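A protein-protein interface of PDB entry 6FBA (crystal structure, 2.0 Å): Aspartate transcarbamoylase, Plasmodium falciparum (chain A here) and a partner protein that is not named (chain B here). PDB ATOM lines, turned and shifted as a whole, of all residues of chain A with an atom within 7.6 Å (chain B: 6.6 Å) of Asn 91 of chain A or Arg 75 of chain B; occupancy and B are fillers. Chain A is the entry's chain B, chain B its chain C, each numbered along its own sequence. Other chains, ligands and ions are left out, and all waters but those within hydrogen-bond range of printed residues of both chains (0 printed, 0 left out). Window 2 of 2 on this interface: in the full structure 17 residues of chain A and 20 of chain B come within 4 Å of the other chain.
The backbone carbonyl oxygen (O) of Asn 91 of chain A lies within hydrogen-bond range of the guanidinium group (NH2) of Arg 75 of chain B (3.0 Å).
SG of Cys 64 of chain A lies close to O of Leu 90 of chain A, at 3.7 Å.
OG of Ser 65 of chain A is in hydrogen-bond range of ND2 of Asn 91 of chain A (3.4 Å).
N of Phe 67 of chain A is in hydrogen-bond range of O of Ile 92 of chain A (2.9 Å).
The side-chain carboxylate of Asp 79 of chain A is in hydrogen-bond range of the side-chain amide nitrogen of Asn 91 of chain A, at 3.1 Å.
The side-chain carboxylate (OD2) of Asp 79 of chain B lies within salt-bridge range of the guanidinium group (NH1) of Arg 75 of chain B, at 2.8 Å.
OD2 of Asp 79 of chain B sits close to OD1 of Asn 91 of chain B, at 3.2 Å.
Among the printed residues, pairs that only touch across the chains: Ile 92 of chain A with Cys 76 of chain B (3.5 Å), Leu 90 of chain A with Cys 76 of chain B (3.7 Å), Leu 90 of chain A with Ala 80 of chain B (3.9 Å) and Leu 90 of chain A with Asp 79 of chain B (3.999 Å).
Printed residues of chain B within 4 Å of Ile 92 of chain A: Cys 76 (3.5 Å).
Of the printed residues of chain A, Ala 80 of chain B touches Leu 90.
Of the printed residues of chain A, Asp 79 of chain B touches Leu 90.
Of the printed residues of chain B, Leu 90 of chain A touches Cys 76 (3.7 Å), Asp 79 (3.999 Å) and Ala 80 (3.9 Å).
Printed residues of chain B that touch a printed residue of chain A: Arg 75, Cys 76, Asp 79 and Ala 80.
Hydrophobic or aromatic side chains of chain A within 4 Å of the printed part of chain B: Leu 90 and Ile 92.
Along chain A the printed residues that touch a printed residue of chain B span positions 90 to 92.
Among the printed residues, 5 pairs touch across the chains.
Among the printed residues, no Asp or Glu carboxylate lies within 4 Å of a Lys or Arg side-chain nitrogen of the other chain.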
ATOM      1  N   PHE A  63       6.320  26.980  32.764  1.00  0.00           N
ATOM      2  CA  PHE A  63       5.037  26.584  33.308  1.00  0.00           C
ATOM      3  C   PHE A  63       3.976  26.252  32.282  1.00  0.00           C
ATOM      4  O   PHE A  63       4.064  26.673  31.112  1.00  0.00           O
ATOM      5  CB  PHE A  63       4.484  27.749  34.144  1.00  0.00           C
ATOM      6  CG  PHE A  63       5.347  28.062  35.353  1.00  0.00           C
ATOM      7  CD1 PHE A  63       5.186  27.365  36.535  1.00  0.00           C
ATOM      8  CD2 PHE A  63       6.357  28.967  35.297  1.00  0.00           C
ATOM      9  CE1 PHE A  63       5.990  27.648  37.661  1.00  0.00           C
ATOM     10  CE2 PHE A  63       7.176  29.216  36.344  1.00  0.00           C
ATOM     11  CZ  PHE A  63       7.039  28.540  37.528  1.00  0.00           C
ATOM     12  N   CYS A  64       2.976  25.474  32.708  1.00  0.00           N
ATOM     13  CA  CYS A  64       1.787  25.281  31.901  1.00  0.00           C
ATOM     14  C   CYS A  64       0.608  25.778  32.678  1.00  0.00           C
ATOM     15  O   CYS A  64       0.425  25.427  33.800  1.00  0.00           O
ATOM     16  CB  CYS A  64       1.597  23.828  31.393  1.00  0.00           C
ATOM     17  SG  CYS A  64       0.073  23.582  30.439  1.00  0.00           S
ATOM     18  N   SER A  65      -0.141  26.690  32.101  1.00  0.00           N
ATOM     19  CA  SER A  65      -1.370  27.201  32.637  1.00  0.00           C
ATOM     20  C   SER A  65      -2.555  26.524  31.985  1.00  0.00           C
ATOM     21  O   SER A  65      -2.793  26.658  30.784  1.00  0.00           O
ATOM     22  CB  SER A  65      -1.359  28.730  32.521  1.00  0.00           C
ATOM     23  OG  SER A  65      -2.670  29.227  32.614  1.00  0.00           O
ATOM     24  N   VAL A  66      -3.295  25.729  32.748  1.00  0.00           N
ATOM     25  CA  VAL A  66      -4.426  25.011  32.263  1.00  0.00           C
ATOM     26  C   VAL A  66      -5.737  25.563  32.802  1.00  0.00           C
ATOM     27  O   VAL A  66      -6.101  25.287  33.942  1.00  0.00           O
ATOM     28  CB  VAL A  66      -4.313  23.513  32.669  1.00  0.00           C
ATOM     29  CG1 VAL A  66      -5.432  22.685  32.013  1.00  0.00           C
ATOM     30  CG2 VAL A  66      -2.973  22.985  32.359  1.00  0.00           C
ATOM     31  N   PHE A  67      -6.477  26.303  32.006  1.00  0.00           N
ATOM     32  CA  PHE A  67      -7.714  26.924  32.423  1.00  0.00           C
ATOM     33  C   PHE A  67      -8.862  26.296  31.672  1.00  0.00           C
ATOM     34  O   PHE A  67      -8.983  26.417  30.415  1.00  0.00           O
ATOM     35  CB  PHE A  67      -7.653  28.426  32.213  1.00  0.00           C
ATOM     36  CG  PHE A  67      -6.947  29.129  33.294  1.00  0.00           C
ATOM     37  CD1 PHE A  67      -5.633  28.831  33.645  1.00  0.00           C
ATOM     38  CD2 PHE A  67      -7.666  30.024  34.147  1.00  0.00           C
ATOM     39  CE1 PHE A  67      -5.031  29.481  34.658  1.00  0.00           C
ATOM     40  CE2 PHE A  67      -7.038  30.666  35.202  1.00  0.00           C
ATOM     41  CZ  PHE A  67      -5.721  30.378  35.467  1.00  0.00           C
ATOM     42  N   ARG A  75      -6.411  34.130  34.863  1.00  0.00           N
ATOM     43  CA  ARG A  75      -5.383  33.542  34.012  1.00  0.00           C
ATOM     44  C   ARG A  75      -4.327  34.578  33.647  1.00  0.00           C
ATOM     45  O   ARG A  75      -3.183  34.283  33.685  1.00  0.00           O
ATOM     46  CB  ARG A  75      -5.981  32.936  32.716  1.00  0.00           C
ATOM     47  CG  ARG A  75      -4.867  32.672  31.697  1.00  0.00           C
ATOM     48  CD  ARG A  75      -5.231  32.198  30.391  1.00  0.00           C
ATOM     49  NE  ARG A  75      -5.829  33.211  29.514  1.00  0.00           N
ATOM     50  CZ  ARG A  75      -5.225  34.235  28.912  1.00  0.00           C
ATOM     51  NH1 ARG A  75      -3.945  34.537  29.044  1.00  0.00           N
ATOM     52  NH2 ARG A  75      -5.968  34.957  28.138  1.00  0.00           N
ATOM     53  N   CYS A  76      -4.756  35.773  33.237  1.00  0.00           N
ATOM     54  CA  CYS A  76      -3.810  36.887  32.951  1.00  0.00           C
ATOM     55  C   CYS A  76      -2.990  37.265  34.134  1.00  0.00           C
ATOM     56  O   CYS A  76      -1.833  37.609  33.961  1.00  0.00           O
ATOM     57  CB  CYS A  76      -4.539  38.130  32.406  1.00  0.00           C
ATOM     58  SG  CYS A  76      -5.163  37.822  30.759  1.00  0.00           S
ATOM     59  N   PHE A  78      -1.878  35.350  36.701  1.00  0.00           N
ATOM     60  CA  PHE A  78      -0.827  34.413  36.825  1.00  0.00           C
ATOM     61  C   PHE A  78       0.157  34.502  35.706  1.00  0.00           C
ATOM     62  O   PHE A  78       1.391  34.410  35.993  1.00  0.00           O
ATOM     63  CB  PHE A  78      -1.377  32.989  36.887  1.00  0.00           C
ATOM     64  CG  PHE A  78      -1.769  32.586  38.243  1.00  0.00           C
ATOM     65  CD1 PHE A  78      -0.822  32.166  39.101  1.00  0.00           C
ATOM     66  CD2 PHE A  78      -3.080  32.633  38.618  1.00  0.00           C
ATOM     67  CE1 PHE A  78      -1.172  31.782  40.388  1.00  0.00           C
ATOM     68  CE2 PHE A  78      -3.473  32.277  39.901  1.00  0.00           C
ATOM     69  CZ  PHE A  78      -2.503  31.844  40.792  1.00  0.00           C
ATOM     70  N   ASP A  79      -0.299  34.676  34.457  1.00  0.00           N
ATOM     71  CA  ASP A  79       0.685  34.772  33.369  1.00  0.00           C
ATOM     72  C   ASP A  79       1.610  35.973  33.591  1.00  0.00           C
ATOM     73  O   ASP A  79       2.792  35.872  33.400  1.00  0.00           O
ATOM     74  CB  ASP A  79       0.067  34.932  31.955  1.00  0.00           C
ATOM     75  CG  ASP A  79      -0.691  33.674  31.379  1.00  0.00           C
ATOM     76  OD1 ASP A  79      -0.572  32.558  31.854  1.00  0.00           O
ATOM     77  OD2 ASP A  79      -1.523  33.905  30.412  1.00  0.00           O
ATOM     78  N   ILE A  82       4.193  35.086  36.138  1.00  0.00           N
ATOM     79  CA  ILE A  82       5.233  34.166  35.624  1.00  0.00           C
ATOM     80  C   ILE A  82       6.246  34.904  34.767  1.00  0.00           C
ATOM     81  O   ILE A  82       7.477  34.749  34.898  1.00  0.00           O
ATOM     82  CB  ILE A  82       4.558  33.012  34.816  1.00  0.00           C
ATOM     83  CG1 ILE A  82       3.764  32.094  35.707  1.00  0.00           C
ATOM     84  CG2 ILE A  82       5.563  32.174  34.001  1.00  0.00           C
ATOM     85  CD1 ILE A  82       2.702  31.272  34.960  1.00  0.00           C
ATOM     86  N   LEU A  83       5.699  35.699  33.815  1.00  0.00           N
ATOM     87  CA  LEU A  83       6.544  36.425  32.878  1.00  0.00           C
ATOM     88  C   LEU A  83       7.365  37.513  33.542  1.00  0.00           C
ATOM     89  O   LEU A  83       8.523  37.781  33.161  1.00  0.00           O
ATOM     90  CB  LEU A  83       5.718  36.984  31.734  1.00  0.00           C
ATOM     91  CG  LEU A  83       4.817  35.973  30.979  1.00  0.00           C
ATOM     92  CD1 LEU A  83       3.757  36.705  30.178  1.00  0.00           C
ATOM     93  CD2 LEU A  83       5.704  35.047  30.074  1.00  0.00           C
ATOM     94  N   VAL A  89       5.593  30.512  29.913  1.00  0.00           N
ATOM     95  CA  VAL A  89       4.367  29.803  30.117  1.00  0.00           C
ATOM     96  C   VAL A  89       3.733  29.378  28.774  1.00  0.00           C
ATOM     97  O   VAL A  89       3.804  30.123  27.776  1.00  0.00           O
ATOM     98  CB  VAL A  89       3.377  30.641  30.923  1.00  0.00           C
ATOM     99  CG1 VAL A  89       2.949  31.914  30.211  1.00  0.00           C
ATOM    100  CG2 VAL A  89       2.153  29.802  31.251  1.00  0.00           C
ATOM    101  N   LEU A  90       3.247  28.139  28.758  1.00  0.00           N
ATOM    102  CA  LEU A  90       2.346  27.724  27.686  1.00  0.00           C
ATOM    103  C   LEU A  90       0.960  27.486  28.227  1.00  0.00           C
ATOM    104  O   LEU A  90       0.770  27.095  29.393  1.00  0.00           O
ATOM    105  CB  LEU A  90       2.842  26.490  26.883  1.00  0.00           C
ATOM    106  CG  LEU A  90       3.063  25.285  27.753  1.00  0.00           C
ATOM    107  CD1 LEU A  90       2.295  24.077  27.228  1.00  0.00           C
ATOM    108  CD2 LEU A  90       4.543  24.995  27.783  1.00  0.00           C
ATOM    109  N   ASN A  91      -0.020  27.892  27.446  1.00  0.00           N
ATOM    110  CA  ASN A  91      -1.395  28.026  27.908  1.00  0.00           C
ATOM    111  C   ASN A  91      -2.282  26.952  27.237  1.00  0.00           C
ATOM    112  O   ASN A  91      -2.136  26.666  26.031  1.00  0.00           O
ATOM    113  CB  ASN A  91      -1.936  29.428  27.572  1.00  0.00           C
ATOM    114  CG  ASN A  91      -1.296  30.497  28.375  1.00  0.00           C
ATOM    115  OD1 ASN A  91      -0.440  31.231  27.862  1.00  0.00           O
ATOM    116  ND2 ASN A  91      -1.696  30.646  29.641  1.00  0.00           N
ATOM    117  N   ILE A  92      -3.100  26.308  28.048  1.00  0.00           N
ATOM    118  CA  ILE A  92      -4.186  25.461  27.604  1.00  0.00           C
ATOM    119  C   ILE A  92      -5.482  26.160  28.080  1.00  0.00           C
ATOM    120  O   ILE A  92      -5.661  26.384  29.254  1.00  0.00           O
ATOM    121  CB  ILE A  92      -4.130  24.050  28.129  1.00  0.00           C
ATOM    122  CG1 ILE A  92      -2.893  23.349  27.560  1.00  0.00           C
ATOM    123  CG2 ILE A  92      -5.423  23.260  27.779  1.00  0.00           C
ATOM    124  CD1 ILE A  92      -2.681  21.992  28.144  1.00  0.00           C
ATOM    125  N   THR A  93      -6.404  26.429  27.182  1.00  0.00           N
ATOM    126  CA  THR A  93      -7.395  27.420  27.458  1.00  0.00           C
ATOM    127  C   THR A  93      -8.813  27.203  26.952  1.00  0.00           C
ATOM    128  O   THR A  93      -9.365  28.131  26.427  1.00  0.00           O
ATOM    129  CB  THR A  93      -6.778  28.741  27.046  1.00  0.00           C
ATOM    130  OG1 THR A  93      -7.264  29.730  27.893  1.00  0.00           O
ATOM    131  CG2 THR A  93      -6.965  29.094  25.639  1.00  0.00           C
ATOM    132  N   ASP A  94      -9.467  26.070  27.277  1.00  0.00           N
ATOM    133  CA  ASP A  94     -10.896  25.808  26.828  1.00  0.00           C
ATOM    134  C   ASP A  94     -12.092  25.774  27.797  1.00  0.00           C
ATOM    135  O   ASP A  94     -11.967  25.920  29.009  1.00  0.00           O
ATOM    136  CB  ASP A  94     -11.014  24.681  25.755  1.00  0.00           C
ATOM    137  CG  ASP A  94     -10.019  23.596  25.931  1.00  0.00           C
ATOM    138  OD1 ASP A  94     -10.174  23.029  27.008  1.00  0.00           O
ATOM    139  OD2 ASP A  94      -9.092  23.304  25.063  1.00  0.00           O
ATOM    140  N   SER B  65       3.809  28.628  15.847  1.00  0.00           N
ATOM    141  CA  SER B  65       3.230  27.328  15.863  1.00  0.00           C
ATOM    142  C   SER B  65       1.822  27.498  15.332  1.00  0.00           C
ATOM    143  O   SER B  65       1.011  28.165  15.929  1.00  0.00           O
ATOM    144  CB  SER B  65       3.313  26.783  17.302  1.00  0.00           C
ATOM    145  OG  SER B  65       2.316  25.852  17.502  1.00  0.00           O
ATOM    146  N   VAL B  66       1.521  26.902  14.186  1.00  0.00           N
ATOM    147  CA  VAL B  66       0.201  26.972  13.531  1.00  0.00           C
ATOM    148  C   VAL B  66      -0.473  25.633  13.541  1.00  0.00           C
ATOM    149  O   VAL B  66      -0.035  24.702  12.856  1.00  0.00           O
ATOM    150  CB  VAL B  66       0.402  27.397  12.052  1.00  0.00           C
ATOM    151  CG1 VAL B  66      -0.873  27.488  11.307  1.00  0.00           C
ATOM    152  CG2 VAL B  66       1.257  28.625  11.942  1.00  0.00           C
ATOM    153  N   PHE B  67      -1.536  25.494  14.291  1.00  0.00           N
ATOM    154  CA  PHE B  67      -2.185  24.217  14.488  1.00  0.00           C
ATOM    155  C   PHE B  67      -3.633  24.436  14.083  1.00  0.00           C
ATOM    156  O   PHE B  67      -4.371  25.180  14.737  1.00  0.00           O
ATOM    157  CB  PHE B  67      -2.103  23.730  15.926  1.00  0.00           C
ATOM    158  CG  PHE B  67      -0.833  23.029  16.255  1.00  0.00           C
ATOM    159  CD1 PHE B  67       0.417  23.648  16.211  1.00  0.00           C
ATOM    160  CD2 PHE B  67      -0.874  21.691  16.597  1.00  0.00           C
ATOM    161  CE1 PHE B  67       1.560  22.913  16.550  1.00  0.00           C
ATOM    162  CE2 PHE B  67       0.264  20.983  16.873  1.00  0.00           C
ATOM    163  CZ  PHE B  67       1.469  21.590  16.801  1.00  0.00           C
ATOM    164  N   SER B  71      -5.481  19.622  18.269  1.00  0.00           N
ATOM    165  CA  SER B  71      -4.385  18.738  18.578  1.00  0.00           C
ATOM    166  C   SER B  71      -3.609  19.413  19.737  1.00  0.00           C
ATOM    167  O   SER B  71      -2.403  19.749  19.617  1.00  0.00           O
ATOM    168  CB  SER B  71      -3.488  18.671  17.350  1.00  0.00           C
ATOM    169  OG  SER B  71      -3.378  20.119  16.970  1.00  0.00           O
ATOM    170  N   THR B  72      -4.306  19.608  20.856  1.00  0.00           N
ATOM    171  CA  THR B  72      -3.703  20.412  21.882  1.00  0.00           C
ATOM    172  C   THR B  72      -2.434  19.731  22.556  1.00  0.00           C
ATOM    173  O   THR B  72      -1.448  20.373  22.770  1.00  0.00           O
ATOM    174  CB  THR B  72      -4.757  21.097  22.819  1.00  0.00           C
ATOM    175  OG1 THR B  72      -4.481  20.792  24.192  1.00  0.00           O
ATOM    176  CG2 THR B  72      -6.083  20.889  22.426  1.00  0.00           C
ATOM    177  N   ARG B  73      -2.422  18.432  22.747  1.00  0.00           N
ATOM    178  CA  ARG B  73      -1.259  17.690  23.275  1.00  0.00           C
ATOM    179  C   ARG B  73      -0.007  17.817  22.443  1.00  0.00           C
ATOM    180  O   ARG B  73       1.073  18.057  22.945  1.00  0.00           O
ATOM    181  CB  ARG B  73      -1.641  16.232  23.397  1.00  0.00           C
ATOM    182  CG  ARG B  73      -2.769  16.021  24.417  1.00  0.00           C
ATOM    183  CD  ARG B  73      -3.463  14.631  24.389  1.00  0.00           C
ATOM    184  NE  ARG B  73      -4.328  14.465  25.552  1.00  0.00           N
ATOM    185  CZ  ARG B  73      -5.518  15.055  25.697  1.00  0.00           C
ATOM    186  NH1 ARG B  73      -6.186  14.890  26.817  1.00  0.00           N
ATOM    187  NH2 ARG B  73      -6.022  15.883  24.758  1.00  0.00           N
ATOM    188  N   THR B  74      -0.149  17.740  21.129  1.00  0.00           N
ATOM    189  CA  THR B  74       1.031  17.877  20.298  1.00  0.00           C
ATOM    190  C   THR B  74       1.564  19.276  20.276  1.00  0.00           C
ATOM    191  O   THR B  74       2.775  19.502  20.328  1.00  0.00           O
ATOM    192  CB  THR B  74       0.713  17.412  18.786  1.00  0.00           C
ATOM    193  OG1 THR B  74       0.150  16.108  18.832  1.00  0.00           O
ATOM    194  CG2 THR B  74       1.935  17.519  17.906  1.00  0.00           C
ATOM    195  N   ARG B  75       0.626  20.202  20.167  1.00  0.00           N
ATOM    196  CA  ARG B  75       0.974  21.596  20.235  1.00  0.00           C
ATOM    197  C   ARG B  75       1.713  21.990  21.508  1.00  0.00           C
ATOM    198  O   ARG B  75       2.748  22.660  21.415  1.00  0.00           O
ATOM    199  CB  ARG B  75      -0.338  22.354  20.068  1.00  0.00           C
ATOM    200  CG  ARG B  75      -0.174  23.802  19.711  1.00  0.00           C
ATOM    201  CD  ARG B  75      -0.174  24.655  20.916  1.00  0.00           C
ATOM    202  NE  ARG B  75      -1.473  24.693  21.621  1.00  0.00           N
ATOM    203  CZ  ARG B  75      -1.542  25.193  22.870  1.00  0.00           C
ATOM    204  NH1 ARG B  75      -0.437  25.750  23.443  1.00  0.00           N
ATOM    205  NH2 ARG B  75      -2.658  25.204  23.520  1.00  0.00           N
ATOM    206  N   CYS B  76       1.222  21.548  22.667  1.00  0.00           N
ATOM    207  CA  CYS B  76       1.918  21.739  23.941  1.00  0.00           C
ATOM    208  C   CYS B  76       3.241  21.063  24.036  1.00  0.00           C
ATOM    209  O   CYS B  76       4.179  21.651  24.569  1.00  0.00           O
ATOM    210  CB  CYS B  76       1.045  21.252  25.073  1.00  0.00           C
ATOM    211  SG  CYS B  76      -0.385  22.331  25.302  1.00  0.00           S
ATOM    212  N   SER B  77       3.428  19.880  23.444  1.00  0.00           N
ATOM    213  CA  SER B  77       4.766  19.270  23.400  1.00  0.00           C
ATOM    214  C   SER B  77       5.767  20.081  22.673  1.00  0.00           C
ATOM    215  O   SER B  77       6.896  20.207  23.122  1.00  0.00           O
ATOM    216  CB  SER B  77       4.670  17.860  22.711  1.00  0.00           C
ATOM    217  OG  SER B  77       3.507  17.191  23.184  1.00  0.00           O
ATOM    218  N   PHE B  78       5.393  20.582  21.460  1.00  0.00           N
ATOM    219  CA  PHE B  78       6.297  21.513  20.777  1.00  0.00           C
ATOM    220  C   PHE B  78       6.573  22.815  21.508  1.00  0.00           C
ATOM    221  O   PHE B  78       7.717  23.280  21.569  1.00  0.00           O
ATOM    222  CB  PHE B  78       5.774  21.778  19.338  1.00  0.00           C
ATOM    223  CG  PHE B  78       6.188  20.703  18.369  1.00  0.00           C
ATOM    224  CD1 PHE B  78       7.418  20.758  17.811  1.00  0.00           C
ATOM    225  CD2 PHE B  78       5.359  19.695  18.035  1.00  0.00           C
ATOM    226  CE1 PHE B  78       7.825  19.813  16.874  1.00  0.00           C
ATOM    227  CE2 PHE B  78       5.757  18.727  17.111  1.00  0.00           C
ATOM    228  CZ  PHE B  78       7.005  18.792  16.547  1.00  0.00           C
ATOM    229  N   ASP B  79       5.533  23.421  22.078  1.00  0.00           N
ATOM    230  CA  ASP B  79       5.721  24.668  22.879  1.00  0.00           C
ATOM    231  C   ASP B  79       6.690  24.419  24.072  1.00  0.00           C
ATOM    232  O   ASP B  79       7.602  25.185  24.259  1.00  0.00           O
ATOM    233  CB  ASP B  79       4.406  25.247  23.419  1.00  0.00           C
ATOM    234  CG  ASP B  79       3.484  25.967  22.353  1.00  0.00           C
ATOM    235  OD1 ASP B  79       3.878  26.086  21.156  1.00  0.00           O
ATOM    236  OD2 ASP B  79       2.273  26.287  22.792  1.00  0.00           O
ATOM    237  N   ALA B  80       6.493  23.332  24.844  1.00  0.00           N
ATOM    238  CA  ALA B  80       7.388  23.034  25.894  1.00  0.00           C
ATOM    239  C   ALA B  80       8.853  22.920  25.409  1.00  0.00           C
ATOM    240  O   ALA B  80       9.765  23.503  26.045  1.00  0.00           O
ATOM    241  CB  ALA B  80       6.972  21.761  26.591  1.00  0.00           C
ATOM    242  N   ASN B  91       1.404  31.633  18.708  1.00  0.00           N
ATOM    243  CA  ASN B  91       0.539  30.550  18.464  1.00  0.00           C
ATOM    244  C   ASN B  91      -0.621  30.973  17.623  1.00  0.00           C
ATOM    245  O   ASN B  91      -1.338  31.908  17.964  1.00  0.00           O
ATOM    246  CB  ASN B  91       0.032  29.924  19.747  1.00  0.00           C
ATOM    247  CG  ASN B  91       1.114  29.191  20.506  1.00  0.00           C
ATOM    248  OD1 ASN B  91       1.409  28.032  20.280  1.00  0.00           O
ATOM    249  ND2 ASN B  91       1.690  29.866  21.443  1.00  0.00           N
ATOM    250  N   ILE B  92      -0.846  30.202  16.557  1.00  0.00           N
ATOM    251  CA  ILE B  92      -2.110  30.265  15.816  1.00  0.00           C
ATOM    252  C   ILE B  92      -2.805  28.928  16.043  1.00  0.00           C
ATOM    253  O   ILE B  92      -2.226  27.890  15.705  1.00  0.00           O
ATOM    254  CB  ILE B  92      -1.850  30.525  14.344  1.00  0.00           C
ATOM    255  CG1 ILE B  92      -1.290  31.900  14.177  1.00  0.00           C
ATOM    256  CG2 ILE B  92      -3.132  30.312  13.536  1.00  0.00           C
ATOM    257  CD1 ILE B  92      -0.702  32.185  12.799  1.00  0.00           C
ATOM    258  N   THR B  93      -4.023  28.937  16.542  1.00  0.00           N
ATOM    259  CA  THR B  93      -4.723  27.733  16.702  1.00  0.00           C
ATOM    260  C   THR B  93      -6.139  27.918  16.193  1.00  0.00           C
ATOM    261  O   THR B  93      -6.777  28.854  16.481  1.00  0.00           O
ATOM    262  CB  THR B  93      -4.750  27.226  18.165  1.00  0.00           C
ATOM    263  OG1 THR B  93      -5.418  28.204  18.947  1.00  0.00           O
ATOM    264  CG2 THR B  93      -3.411  27.155  18.681  1.00  0.00           C
ATOM    265  N   ALA B 144       4.073  18.833  12.174  1.00  0.00           N
ATOM    266  CA  ALA B 144       3.679  18.224  13.433  1.00  0.00           C
ATOM    267  C   ALA B 144       2.586  17.197  13.230  1.00  0.00           C
ATOM    268  O   ALA B 144       1.951  16.802  14.231  1.00  0.00           O
ATOM    269  CB  ALA B 144       3.140  19.319  14.383  1.00  0.00           C
